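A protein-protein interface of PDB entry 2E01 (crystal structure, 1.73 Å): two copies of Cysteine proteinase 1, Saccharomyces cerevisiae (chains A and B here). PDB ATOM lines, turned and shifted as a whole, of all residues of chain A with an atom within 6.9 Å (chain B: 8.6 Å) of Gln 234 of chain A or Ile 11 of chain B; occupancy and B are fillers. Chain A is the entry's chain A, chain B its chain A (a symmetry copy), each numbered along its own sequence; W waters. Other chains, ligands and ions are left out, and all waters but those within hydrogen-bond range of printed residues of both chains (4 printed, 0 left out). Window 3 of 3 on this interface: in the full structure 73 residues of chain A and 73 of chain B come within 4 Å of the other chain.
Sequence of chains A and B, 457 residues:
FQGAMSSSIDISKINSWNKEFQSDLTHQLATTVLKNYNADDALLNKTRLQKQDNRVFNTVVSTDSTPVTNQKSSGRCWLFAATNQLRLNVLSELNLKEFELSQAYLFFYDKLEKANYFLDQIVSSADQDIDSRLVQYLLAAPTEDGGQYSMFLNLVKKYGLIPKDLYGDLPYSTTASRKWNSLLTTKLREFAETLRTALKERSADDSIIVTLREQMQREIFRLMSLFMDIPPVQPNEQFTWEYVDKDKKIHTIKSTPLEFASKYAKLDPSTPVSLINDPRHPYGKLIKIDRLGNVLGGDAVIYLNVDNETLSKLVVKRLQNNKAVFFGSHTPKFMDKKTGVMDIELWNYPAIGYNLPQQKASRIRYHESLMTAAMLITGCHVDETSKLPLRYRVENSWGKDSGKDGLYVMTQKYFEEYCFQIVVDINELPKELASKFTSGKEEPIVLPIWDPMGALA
O of Ile 9 of chain B sits at hydrogen-bond distance from NZ of Lys 158 of chain A, at 2.9 Å.
OH of Tyr 159 of chain A sits at hydrogen-bond distance from OE2 of Glu 113 of chain A (2.6 Å).
OH of Tyr 105 of chain A sits at hydrogen-bond distance from O of Tyr 159 of chain A (2.6 Å).
The backbone carbonyl oxygen (O) of Ile 11 of chain B lies within hydrogen-bond range of the side-chain amide nitrogen (ND2) of Asn 15 of chain B (3.0 Å).
O of Pro 235 of chain A lies within hydrogen-bond range of N of Leu 258 of chain A (3.1 Å).
The side-chain carboxylate (OE2) of Glu 113 of chain A lies within salt-bridge range of the side-chain amino group (NZ) of Lys 158 of chain A, at 2.8 Å.
The backbone NH (N) of Gln 234 of chain A is in hydrogen-bond range of the side-chain carboxylate (OE1) of Glu 237 of chain A (2.8 Å).
Among the printed residues, merely in contact across the chains: Glu 113 of chain A with Ile 9 of chain B, Tyr 159 of chain A with Ile 9 of chain B, Tyr 159 of chain A with Ile 11 of chain B, Ile 230 of chain A with Ile 14 of chain B, Ile 230 of chain A with Asn 15 of chain B, Ile 230 of chain A with Asn 18 of chain B, Gln 234 of chain A with Ile 11 of chain B, Gln 234 of chain A with Asn 15 of chain B and Pro 235 of chain A with Ile 11 of chain B.
Printed residues of chain B within 4 Å of Glu 113 of chain A: Ile 9 (3.5 Å).
Printed residues of chain B within 4 Å of Tyr 159 of chain A: Ile 9 and Ile 11.
Pro 232 of chain A touches none of the printed residues of chain B.
No residue of chain B comes within 4 Å of Val 233 of chain A.
Of chain B, only Ile 11 (3.8 Å) and Asn 15 (3.5 Å) come within 4 Å of Gln 234 of chain A.
The nearest residue of chain B that does not touch Gln 234 of chain A is Ser 12 of chain B (4.8 Å).
The nearest residue of chain A that does not touch Ile 11 of chain B is Lys 158 of chain A (4.3 Å).
The nearest printed residue of chain B that does not touch Tyr 159 of chain A is Ile 14 of chain B (5.1 Å).
Hydrophobic or aromatic side chains of chain A that line the printed part of chain B: Tyr 159, Ile 230 and Pro 235.
Of the 11 printed residues of chain B, 5 touch a printed residue of chain A.
Among the printed residues, 10 pairs touch across the chains.
Among the printed residues, no Asp or Glu carboxylate lies within 4 Å of a Lys or Arg side-chain nitrogen of the other chain.
No position is printed for both chains.
Of the 10 pairs that touch across the chains among the printed residues, none has its exchanged pair printed and touching as well.
Water W1 lies within hydrogen-bond range of the side-chain carboxylate (OE1) of Glu 113 of chain A (2.7 Å), the backbone NH (N) of Ile 9 of chain B (2.8 Å) and the side-chain amino group (NZ) of Lys 158 of chain A (3.0 Å).
Water W4 lies within hydrogen-bond range of O of Pro 231 of chain A (2.7 Å) and OD1 of Asn 15 of chain B (2.8 Å).
Water W3 bridges the side-chain amide oxygen (OD1) of Asn 18 of chain B (2.7 Å) and the backbone NH (N) of Ile 230 of chain A (2.8 Å).
Water W2 lies within hydrogen-bond range of the side-chain hydroxyl (OH) of Tyr 109 of chain A (2.7 Å) and the side-chain amide nitrogen (ND2) of Asn 15 of chain B (2.9 Å).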
ATOM      1  N   TYR A 105      -6.711 -12.059 -11.403  1.00  0.00           N
ATOM      2  CA  TYR A 105      -7.945 -12.667 -10.914  1.00  0.00           C
ATOM      3  C   TYR A 105      -7.678 -13.569  -9.706  1.00  0.00           C
ATOM      4  O   TYR A 105      -8.356 -13.475  -8.652  1.00  0.00           O
ATOM      5  CB  TYR A 105      -8.522 -13.470 -12.052  1.00  0.00           C
ATOM      6  CG  TYR A 105      -9.832 -14.165 -11.756  1.00  0.00           C
ATOM      7  CD1 TYR A 105     -11.031 -13.465 -11.809  1.00  0.00           C
ATOM      8  CD2 TYR A 105      -9.861 -15.517 -11.497  1.00  0.00           C
ATOM      9  CE1 TYR A 105     -12.294 -14.126 -11.615  1.00  0.00           C
ATOM     10  CE2 TYR A 105     -11.118 -16.210 -11.301  1.00  0.00           C
ATOM     11  CZ  TYR A 105     -12.311 -15.489 -11.362  1.00  0.00           C
ATOM     12  OH  TYR A 105     -13.548 -16.118 -11.169  1.00  0.00           O
ATOM     13  N   TYR A 109      -8.382 -12.897  -5.324  1.00  0.00           N
ATOM     14  CA  TYR A 109      -9.029 -13.851  -4.413  1.00  0.00           C
ATOM     15  C   TYR A 109      -8.057 -14.508  -3.433  1.00  0.00           C
ATOM     16  O   TYR A 109      -8.421 -14.781  -2.293  1.00  0.00           O
ATOM     17  CB  TYR A 109      -9.773 -14.900  -5.220  1.00  0.00           C
ATOM     18  CG  TYR A 109     -11.003 -14.334  -5.899  1.00  0.00           C
ATOM     19  CD1 TYR A 109     -11.983 -13.627  -5.164  1.00  0.00           C
ATOM     20  CD2 TYR A 109     -11.214 -14.557  -7.276  1.00  0.00           C
ATOM     21  CE1 TYR A 109     -13.173 -13.153  -5.798  1.00  0.00           C
ATOM     22  CE2 TYR A 109     -12.378 -14.098  -7.897  1.00  0.00           C
ATOM     23  CZ  TYR A 109     -13.336 -13.420  -7.159  1.00  0.00           C
ATOM     24  OH  TYR A 109     -14.487 -13.086  -7.817  1.00  0.00           O
ATOM     25  N   GLU A 113      -8.887 -14.336   0.490  1.00  0.00           N
ATOM     26  CA  GLU A 113      -9.045 -15.575   1.239  1.00  0.00           C
ATOM     27  C   GLU A 113      -7.981 -15.680   2.336  1.00  0.00           C
ATOM     28  O   GLU A 113      -8.272 -16.113   3.438  1.00  0.00           O
ATOM     29  CB  GLU A 113      -8.907 -16.786   0.329  1.00  0.00           C
ATOM     30  CG  GLU A 113     -10.045 -16.957  -0.694  1.00  0.00           C
ATOM     31  CD  GLU A 113     -11.299 -17.576  -0.070  1.00  0.00           C
ATOM     32  OE1 GLU A 113     -11.249 -18.029   1.091  1.00  0.00           O
ATOM     33  OE2 GLU A 113     -12.335 -17.596  -0.758  1.00  0.00           O
ATOM     34  N   LYS A 158     -12.618 -23.022  -6.486  1.00  0.00           N
ATOM     35  CA  LYS A 158     -13.716 -22.138  -6.036  1.00  0.00           C
ATOM     36  C   LYS A 158     -14.077 -21.036  -7.037  1.00  0.00           C
ATOM     37  O   LYS A 158     -15.262 -20.720  -7.238  1.00  0.00           O
ATOM     38  CB  LYS A 158     -13.343 -21.493  -4.702  1.00  0.00           C
ATOM     39  CG  LYS A 158     -14.365 -20.480  -4.132  1.00  0.00           C
ATOM     40  CD  LYS A 158     -14.055 -20.169  -2.691  1.00  0.00           C
ATOM     41  CE  LYS A 158     -15.057 -19.218  -2.058  1.00  0.00           C
ATOM     42  NZ  LYS A 158     -14.713 -19.002  -0.595  1.00  0.00           N
ATOM     43  N   TYR A 159     -13.052 -20.455  -7.676  1.00  0.00           N
ATOM     44  CA  TYR A 159     -13.226 -19.305  -8.568  1.00  0.00           C
ATOM     45  C   TYR A 159     -13.061 -19.499 -10.054  1.00  0.00           C
ATOM     46  O   TYR A 159     -13.460 -18.649 -10.837  1.00  0.00           O
ATOM     47  CB  TYR A 159     -12.249 -18.199  -8.089  1.00  0.00           C
ATOM     48  CG  TYR A 159     -12.522 -17.743  -6.674  1.00  0.00           C
ATOM     49  CD1 TYR A 159     -13.585 -16.874  -6.398  1.00  0.00           C
ATOM     50  CD2 TYR A 159     -11.707 -18.146  -5.622  1.00  0.00           C
ATOM     51  CE1 TYR A 159     -13.825 -16.409  -5.151  1.00  0.00           C
ATOM     52  CE2 TYR A 159     -11.937 -17.682  -4.319  1.00  0.00           C
ATOM     53  CZ  TYR A 159     -12.998 -16.811  -4.093  1.00  0.00           C
ATOM     54  OH  TYR A 159     -13.251 -16.351  -2.848  1.00  0.00           O
ATOM     55  N   ILE A 162     -10.175 -16.947 -15.862  1.00  0.00           N
ATOM     56  CA  ILE A 162     -10.702 -16.114 -16.930  1.00  0.00           C
ATOM     57  C   ILE A 162      -9.594 -15.526 -17.796  1.00  0.00           C
ATOM     58  O   ILE A 162      -8.457 -15.442 -17.348  1.00  0.00           O
ATOM     59  CB  ILE A 162     -11.528 -14.906 -16.391  1.00  0.00           C
ATOM     60  CG1 ILE A 162     -10.632 -13.983 -15.554  1.00  0.00           C
ATOM     61  CG2 ILE A 162     -12.787 -15.421 -15.621  1.00  0.00           C
ATOM     62  CD1 ILE A 162     -11.410 -12.760 -15.032  1.00  0.00           C
ATOM     63  N   ILE A 230     -13.243  -5.956  -7.578  1.00  0.00           N
ATOM     64  CA  ILE A 230     -13.583  -7.363  -7.484  1.00  0.00           C
ATOM     65  C   ILE A 230     -13.714  -7.778  -8.982  1.00  0.00           C
ATOM     66  O   ILE A 230     -14.058  -6.946  -9.814  1.00  0.00           O
ATOM     67  CB  ILE A 230     -14.943  -7.557  -6.750  1.00  0.00           C
ATOM     68  CG1 ILE A 230     -15.215  -9.056  -6.542  1.00  0.00           C
ATOM     69  CG2 ILE A 230     -16.083  -6.905  -7.559  1.00  0.00           C
ATOM     70  CD1 ILE A 230     -16.403  -9.266  -5.580  1.00  0.00           C
ATOM     71  N   PRO A 231     -13.387  -9.037  -9.339  1.00  0.00           N
ATOM     72  CA  PRO A 231     -13.519  -9.430 -10.749  1.00  0.00           C
ATOM     73  C   PRO A 231     -14.955  -9.134 -11.268  1.00  0.00           C
ATOM     74  O   PRO A 231     -15.917  -9.094 -10.498  1.00  0.00           O
ATOM     75  CB  PRO A 231     -13.131 -10.894 -10.733  1.00  0.00           C
ATOM     76  CG  PRO A 231     -12.014 -10.894  -9.717  1.00  0.00           C
ATOM     77  CD  PRO A 231     -12.589 -10.037  -8.575  1.00  0.00           C
ATOM     78  N   PRO A 232     -15.089  -8.922 -12.592  1.00  0.00           N
ATOM     79  CA  PRO A 232     -16.354  -8.577 -13.233  1.00  0.00           C
ATOM     80  C   PRO A 232     -17.468  -9.599 -13.278  1.00  0.00           C
ATOM     81  O   PRO A 232     -18.594  -9.231 -13.550  1.00  0.00           O
ATOM     82  CB  PRO A 232     -15.900  -8.122 -14.623  1.00  0.00           C
ATOM     83  CG  PRO A 232     -14.803  -9.113 -14.947  1.00  0.00           C
ATOM     84  CD  PRO A 232     -14.051  -9.177 -13.601  1.00  0.00           C
ATOM     85  N   VAL A 233     -17.135 -10.862 -13.056  1.00  0.00           N
ATOM     86  CA  VAL A 233     -18.170 -11.908 -13.055  1.00  0.00           C
ATOM     87  C   VAL A 233     -17.888 -12.866 -11.940  1.00  0.00           C
ATOM     88  O   VAL A 233     -16.729 -13.053 -11.562  1.00  0.00           O
ATOM     89  CB  VAL A 233     -18.220 -12.739 -14.375  1.00  0.00           C
ATOM     90  CG1 VAL A 233     -18.684 -11.843 -15.546  1.00  0.00           C
ATOM     91  CG2 VAL A 233     -16.850 -13.364 -14.652  1.00  0.00           C
ATOM     92  N   GLN A 234     -18.960 -13.453 -11.392  1.00  0.00           N
ATOM     93  CA  GLN A 234     -18.860 -14.449 -10.347  1.00  0.00           C
ATOM     94  C   GLN A 234     -18.432 -15.805 -10.960  1.00  0.00           C
ATOM     95  O   GLN A 234     -18.525 -16.015 -12.179  1.00  0.00           O
ATOM     96  CB  GLN A 234     -20.192 -14.460  -9.571  1.00  0.00           C
ATOM     97  CG  GLN A 234     -20.320 -13.152  -8.811  1.00  0.00           C
ATOM     98  CD  GLN A 234     -21.697 -12.860  -8.246  1.00  0.00           C
ATOM     99  OE1 GLN A 234     -22.261 -13.670  -7.505  1.00  0.00           O
ATOM    100  NE2 GLN A 234     -22.236 -11.696  -8.572  1.00  0.00           N
ATOM    101  N   PRO A 235     -17.976 -16.765 -10.138  1.00  0.00           N
ATOM    102  CA  PRO A 235     -17.492 -18.053 -10.694  1.00  0.00           C
ATOM    103  C   PRO A 235     -18.435 -18.870 -11.547  1.00  0.00           C
ATOM    104  O   PRO A 235     -18.005 -19.531 -12.479  1.00  0.00           O
ATOM    105  CB  PRO A 235     -17.019 -18.829  -9.436  1.00  0.00           C
ATOM    106  CG  PRO A 235     -16.638 -17.727  -8.516  1.00  0.00           C
ATOM    107  CD  PRO A 235     -17.721 -16.680  -8.695  1.00  0.00           C
ATOM    108  N   ASN A 236     -19.724 -18.782 -11.238  1.00  0.00           N
ATOM    109  CA  ASN A 236     -20.734 -19.507 -12.001  1.00  0.00           C
ATOM    110  C   ASN A 236     -21.520 -18.604 -12.919  1.00  0.00           C
ATOM    111  O   ASN A 236     -22.508 -19.042 -13.508  1.00  0.00           O
ATOM    112  CB  ASN A 236     -21.676 -20.225 -11.016  1.00  0.00           C
ATOM    113  CG  ASN A 236     -20.991 -21.389 -10.345  1.00  0.00           C
ATOM    114  OD1 ASN A 236     -20.821 -22.422 -10.937  1.00  0.00           O
ATOM    115  ND2 ASN A 236     -20.579 -21.203  -9.113  1.00  0.00           N
ATOM    116  N   GLU A 237     -21.087 -17.346 -13.037  1.00  0.00           N
ATOM    117  CA  GLU A 237     -21.739 -16.361 -13.881  1.00  0.00           C
ATOM    118  C   GLU A 237     -21.077 -16.326 -15.260  1.00  0.00           C
ATOM    119  O   GLU A 237     -19.853 -16.375 -15.373  1.00  0.00           O
ATOM    120  CB  GLU A 237     -21.673 -14.979 -13.234  1.00  0.00           C
ATOM    121  CG  GLU A 237     -22.184 -13.827 -14.101  1.00  0.00           C
ATOM    122  CD  GLU A 237     -22.094 -12.481 -13.399  1.00  0.00           C
ATOM    123  OE1 GLU A 237     -21.387 -12.366 -12.355  1.00  0.00           O
ATOM    124  OE2 GLU A 237     -22.732 -11.531 -13.890  1.00  0.00           O
ATOM    125  N   GLN A 238     -21.878 -16.216 -16.315  1.00  0.00           N
ATOM    126  CA  GLN A 238     -21.270 -16.205 -17.643  1.00  0.00           C
ATOM    127  C   GLN A 238     -20.588 -14.899 -18.006  1.00  0.00           C
ATOM    128  O   GLN A 238     -21.063 -13.817 -17.658  1.00  0.00           O
ATOM    129  CB  GLN A 238     -22.295 -16.464 -18.754  1.00  0.00           C
ATOM    130  CG  GLN A 238     -22.978 -17.813 -18.712  1.00  0.00           C
ATOM    131  CD  GLN A 238     -23.972 -17.911 -19.875  1.00  0.00           C
ATOM    132  OE1 GLN A 238     -24.800 -17.040 -20.054  1.00  0.00           O
ATOM    133  NE2 GLN A 238     -23.865 -18.963 -20.656  1.00  0.00           N
ATOM    134  N   PHE A 239     -19.460 -15.004 -18.699  1.00  0.00           N
ATOM    135  CA  PHE A 239     -18.830 -13.796 -19.227  1.00  0.00           C
ATOM    136  C   PHE A 239     -18.921 -13.977 -20.729  1.00  0.00           C
ATOM    137  O   PHE A 239     -19.149 -15.101 -21.207  1.00  0.00           O
ATOM    138  CB  PHE A 239     -17.348 -13.659 -18.808  1.00  0.00           C
ATOM    139  CG  PHE A 239     -16.481 -14.848 -19.140  1.00  0.00           C
ATOM    140  CD1 PHE A 239     -16.028 -15.070 -20.442  1.00  0.00           C
ATOM    141  CD2 PHE A 239     -16.032 -15.681 -18.107  1.00  0.00           C
ATOM    142  CE1 PHE A 239     -15.125 -16.108 -20.701  1.00  0.00           C
ATOM    143  CE2 PHE A 239     -15.120 -16.734 -18.345  1.00  0.00           C
ATOM    144  CZ  PHE A 239     -14.664 -16.945 -19.641  1.00  0.00           C
ATOM    145  N   THR A 256     -18.454 -19.525 -18.140  1.00  0.00           N
ATOM    146  CA  THR A 256     -18.329 -18.968 -16.789  1.00  0.00           C
ATOM    147  C   THR A 256     -16.862 -19.229 -16.411  1.00  0.00           C
ATOM    148  O   THR A 256     -16.198 -20.035 -17.049  1.00  0.00           O
ATOM    149  CB  THR A 256     -19.159 -19.741 -15.773  1.00  0.00           C
ATOM    150  OG1 THR A 256     -18.669 -21.099 -15.698  1.00  0.00           O
ATOM    151  CG2 THR A 256     -20.664 -19.712 -16.169  1.00  0.00           C
ATOM    152  N   PRO A 257     -16.348 -18.552 -15.371  1.00  0.00           N
ATOM    153  CA  PRO A 257     -14.953 -18.842 -15.021  1.00  0.00           C
ATOM    154  C   PRO A 257     -14.718 -20.320 -14.677  1.00  0.00           C
ATOM    155  O   PRO A 257     -13.691 -20.884 -15.011  1.00  0.00           O
ATOM    156  CB  PRO A 257     -14.678 -17.932 -13.814  1.00  0.00           C
ATOM    157  CG  PRO A 257     -15.578 -16.706 -14.105  1.00  0.00           C
ATOM    158  CD  PRO A 257     -16.863 -17.379 -14.648  1.00  0.00           C
ATOM    159  N   LEU A 258     -15.671 -20.963 -14.006  1.00  0.00           N
ATOM    160  CA  LEU A 258     -15.464 -22.362 -13.637  1.00  0.00           C
ATOM    161  C   LEU A 258     -15.496 -23.267 -14.865  1.00  0.00           C
ATOM    162  O   LEU A 258     -14.685 -24.189 -14.968  1.00  0.00           O
ATOM    163  CB  LEU A 258     -16.491 -22.786 -12.562  1.00  0.00           C
ATOM    164  CG  LEU A 258     -16.169 -22.204 -11.163  1.00  0.00           C
ATOM    165  CD1 LEU A 258     -17.390 -22.266 -10.216  1.00  0.00           C
ATOM    166  CD2 LEU A 258     -15.035 -23.030 -10.541  1.00  0.00           C
ATOM    167  N   SER B   8     -16.360 -18.547   6.225  1.00  0.00           N
ATOM    168  CA  SER B   8     -15.846 -18.587   4.849  1.00  0.00           C
ATOM    169  C   SER B   8     -16.167 -17.279   4.101  1.00  0.00           C
ATOM    170  O   SER B   8     -17.075 -16.515   4.486  1.00  0.00           O
ATOM    171  CB  SER B   8     -16.494 -19.733   4.066  1.00  0.00           C
ATOM    172  OG  SER B   8     -16.146 -21.003   4.593  1.00  0.00           O
ATOM    173  N   ILE B   9     -15.435 -17.053   3.024  1.00  0.00           N
ATOM    174  CA  ILE B   9     -15.685 -15.926   2.158  1.00  0.00           C
ATOM    175  C   ILE B   9     -16.889 -16.376   1.276  1.00  0.00           C
ATOM    176  O   ILE B   9     -16.811 -17.381   0.537  1.00  0.00           O
ATOM    177  CB  ILE B   9     -14.459 -15.645   1.216  1.00  0.00           C
ATOM    178  CG1 ILE B   9     -13.352 -14.936   2.039  1.00  0.00           C
ATOM    179  CG2 ILE B   9     -14.914 -14.830  -0.010  1.00  0.00           C
ATOM    180  CD1 ILE B   9     -13.828 -13.580   2.595  1.00  0.00           C
ATOM    181  N   ASP B  10     -17.994 -15.649   1.402  1.00  0.00           N
ATOM    182  CA  ASP B  10     -19.180 -16.006   0.591  1.00  0.00           C
ATOM    183  C   ASP B  10     -19.221 -15.071  -0.604  1.00  0.00           C
ATOM    184  O   ASP B  10     -19.159 -13.852  -0.444  1.00  0.00           O
ATOM    185  CB  ASP B  10     -20.457 -15.865   1.415  1.00  0.00           C
ATOM    186  CG  ASP B  10     -21.702 -16.220   0.583  1.00  0.00           C
ATOM    187  OD1 ASP B  10     -22.030 -17.432   0.436  1.00  0.00           O
ATOM    188  OD2 ASP B  10     -22.319 -15.274   0.059  1.00  0.00           O
ATOM    189  N   ILE B  11     -19.331 -15.624  -1.806  1.00  0.00           N
ATOM    190  CA  ILE B  11     -19.294 -14.777  -3.005  1.00  0.00           C
ATOM    191  C   ILE B  11     -20.481 -13.837  -3.097  1.00  0.00           C
ATOM    192  O   ILE B  11     -20.346 -12.701  -3.515  1.00  0.00           O
ATOM    193  CB  ILE B  11     -19.122 -15.654  -4.240  1.00  0.00           C
ATOM    194  CG1 ILE B  11     -17.779 -16.408  -4.089  1.00  0.00           C
ATOM    195  CG2 ILE B  11     -19.185 -14.810  -5.535  1.00  0.00           C
ATOM    196  CD1 ILE B  11     -17.536 -17.483  -5.122  1.00  0.00           C
ATOM    197  N   SER B  12     -21.662 -14.292  -2.696  1.00  0.00           N
ATOM    198  CA  SER B  12     -22.786 -13.365  -2.709  1.00  0.00           C
ATOM    199  C   SER B  12     -22.538 -12.186  -1.768  1.00  0.00           C
ATOM    200  O   SER B  12     -22.821 -11.021  -2.094  1.00  0.00           O
ATOM    201  CB  SER B  12     -24.092 -14.093  -2.282  1.00  0.00           C
ATOM    202  OG  SER B  12     -25.130 -13.121  -2.047  1.00  0.00           O
ATOM    203  N   LYS B  13     -21.994 -12.472  -0.587  1.00  0.00           N
ATOM    204  CA  LYS B  13     -21.738 -11.412   0.385  1.00  0.00           C
ATOM    205  C   LYS B  13     -20.791 -10.347  -0.164  1.00  0.00           C
ATOM    206  O   LYS B  13     -21.072  -9.168  -0.081  1.00  0.00           O
ATOM    207  CB  LYS B  13     -21.085 -12.002   1.649  1.00  0.00           C
ATOM    208  CG  LYS B  13     -21.505 -11.411   2.939  1.00  0.00           C
ATOM    209  CD  LYS B  13     -21.172 -12.350   4.134  1.00  0.00           C
ATOM    210  CE  LYS B  13     -22.115 -13.536   4.198  1.00  0.00           C
ATOM    211  NZ  LYS B  13     -22.098 -14.172   5.580  1.00  0.00           N
ATOM    212  N   ILE B  14     -19.646 -10.781  -0.677  1.00  0.00           N
ATOM    213  CA  ILE B  14     -18.696  -9.773  -1.158  1.00  0.00           C
ATOM    214  C   ILE B  14     -19.221  -9.010  -2.344  1.00  0.00           C
ATOM    215  O   ILE B  14     -18.936  -7.808  -2.479  1.00  0.00           O
ATOM    216  CB  ILE B  14     -17.278 -10.357  -1.436  1.00  0.00           C
ATOM    217  CG1 ILE B  14     -17.335 -11.409  -2.544  1.00  0.00           C
ATOM    218  CG2 ILE B  14     -16.707 -10.961  -0.124  1.00  0.00           C
ATOM    219  CD1 ILE B  14     -15.931 -12.001  -2.963  1.00  0.00           C
ATOM    220  N   ASN B  15     -20.008  -9.652  -3.211  1.00  0.00           N
ATOM    221  CA  ASN B  15     -20.521  -8.872  -4.329  1.00  0.00           C
ATOM    222  C   ASN B  15     -21.649  -7.916  -3.877  1.00  0.00           C
ATOM    223  O   ASN B  15     -21.836  -6.835  -4.466  1.00  0.00           O
ATOM    224  CB  ASN B  15     -21.016  -9.812  -5.441  1.00  0.00           C
ATOM    225  CG  ASN B  15     -19.890 -10.277  -6.336  1.00  0.00           C
ATOM    226  OD1 ASN B  15     -19.583  -9.626  -7.328  1.00  0.00           O
ATOM    227  ND2 ASN B  15     -19.268 -11.418  -5.986  1.00  0.00           N
ATOM    228  N   SER B  16     -22.377  -8.294  -2.827  1.00  0.00           N
ATOM    229  CA  SER B  16     -23.424  -7.419  -2.295  1.00  0.00           C
ATOM    230  C   SER B  16     -22.762  -6.212  -1.602  1.00  0.00           C
ATOM    231  O   SER B  16     -23.159  -5.058  -1.794  1.00  0.00           O
ATOM    232  CB  SER B  16     -24.315  -8.210  -1.342  1.00  0.00           C
ATOM    233  OG  SER B  16     -24.939  -9.267  -2.087  1.00  0.00           O
ATOM    234  N   TRP B  17     -21.725  -6.481  -0.810  1.00  0.00           N
ATOM    235  CA  TRP B  17     -20.989  -5.411  -0.157  1.00  0.00           C
ATOM    236  C   TRP B  17     -20.412  -4.462  -1.223  1.00  0.00           C
ATOM    237  O   TRP B  17     -20.458  -3.245  -1.094  1.00  0.00           O
ATOM    238  CB  TRP B  17     -19.849  -5.998   0.677  1.00  0.00           C
ATOM    239  CG  TRP B  17     -20.322  -6.683   1.888  1.00  0.00           C
ATOM    240  CD1 TRP B  17     -21.523  -6.484   2.551  1.00  0.00           C
ATOM    241  CD2 TRP B  17     -19.624  -7.702   2.608  1.00  0.00           C
ATOM    242  NE1 TRP B  17     -21.603  -7.334   3.646  1.00  0.00           N
ATOM    243  CE2 TRP B  17     -20.449  -8.088   3.701  1.00  0.00           C
ATOM    244  CE3 TRP B  17     -18.372  -8.331   2.435  1.00  0.00           C
ATOM    245  CZ2 TRP B  17     -20.060  -9.073   4.619  1.00  0.00           C
ATOM    246  CZ3 TRP B  17     -17.976  -9.332   3.367  1.00  0.00           C
ATOM    247  CH2 TRP B  17     -18.821  -9.683   4.438  1.00  0.00           C
ATOM    248  N   ASN B  18     -19.846  -5.037  -2.267  1.00  0.00           N
ATOM    249  CA  ASN B  18     -19.272  -4.226  -3.334  1.00  0.00           C
ATOM    250  C   ASN B  18     -20.333  -3.282  -3.914  1.00  0.00           C
ATOM    251  O   ASN B  18     -20.071  -2.121  -4.175  1.00  0.00           O
ATOM    252  CB  ASN B  18     -18.721  -5.105  -4.444  1.00  0.00           C
ATOM    253  CG  ASN B  18     -18.025  -4.290  -5.518  1.00  0.00           C
ATOM    254  OD1 ASN B  18     -17.039  -3.632  -5.232  1.00  0.00           O
ATOM    255  ND2 ASN B  18     -18.554  -4.315  -6.757  1.00  0.00           N
HETATM  256  O   HOH W   1     -13.543 -18.963   2.167  1.00  0.00           O
HETATM  257  O   HOH W   2     -17.141 -12.476  -7.692  1.00  0.00           O
HETATM  258  O   HOH W   3     -14.721  -3.728  -6.655  1.00  0.00           O
HETATM  259  O   HOH W   4     -18.040 -10.426  -9.460  1.00  0.00           O
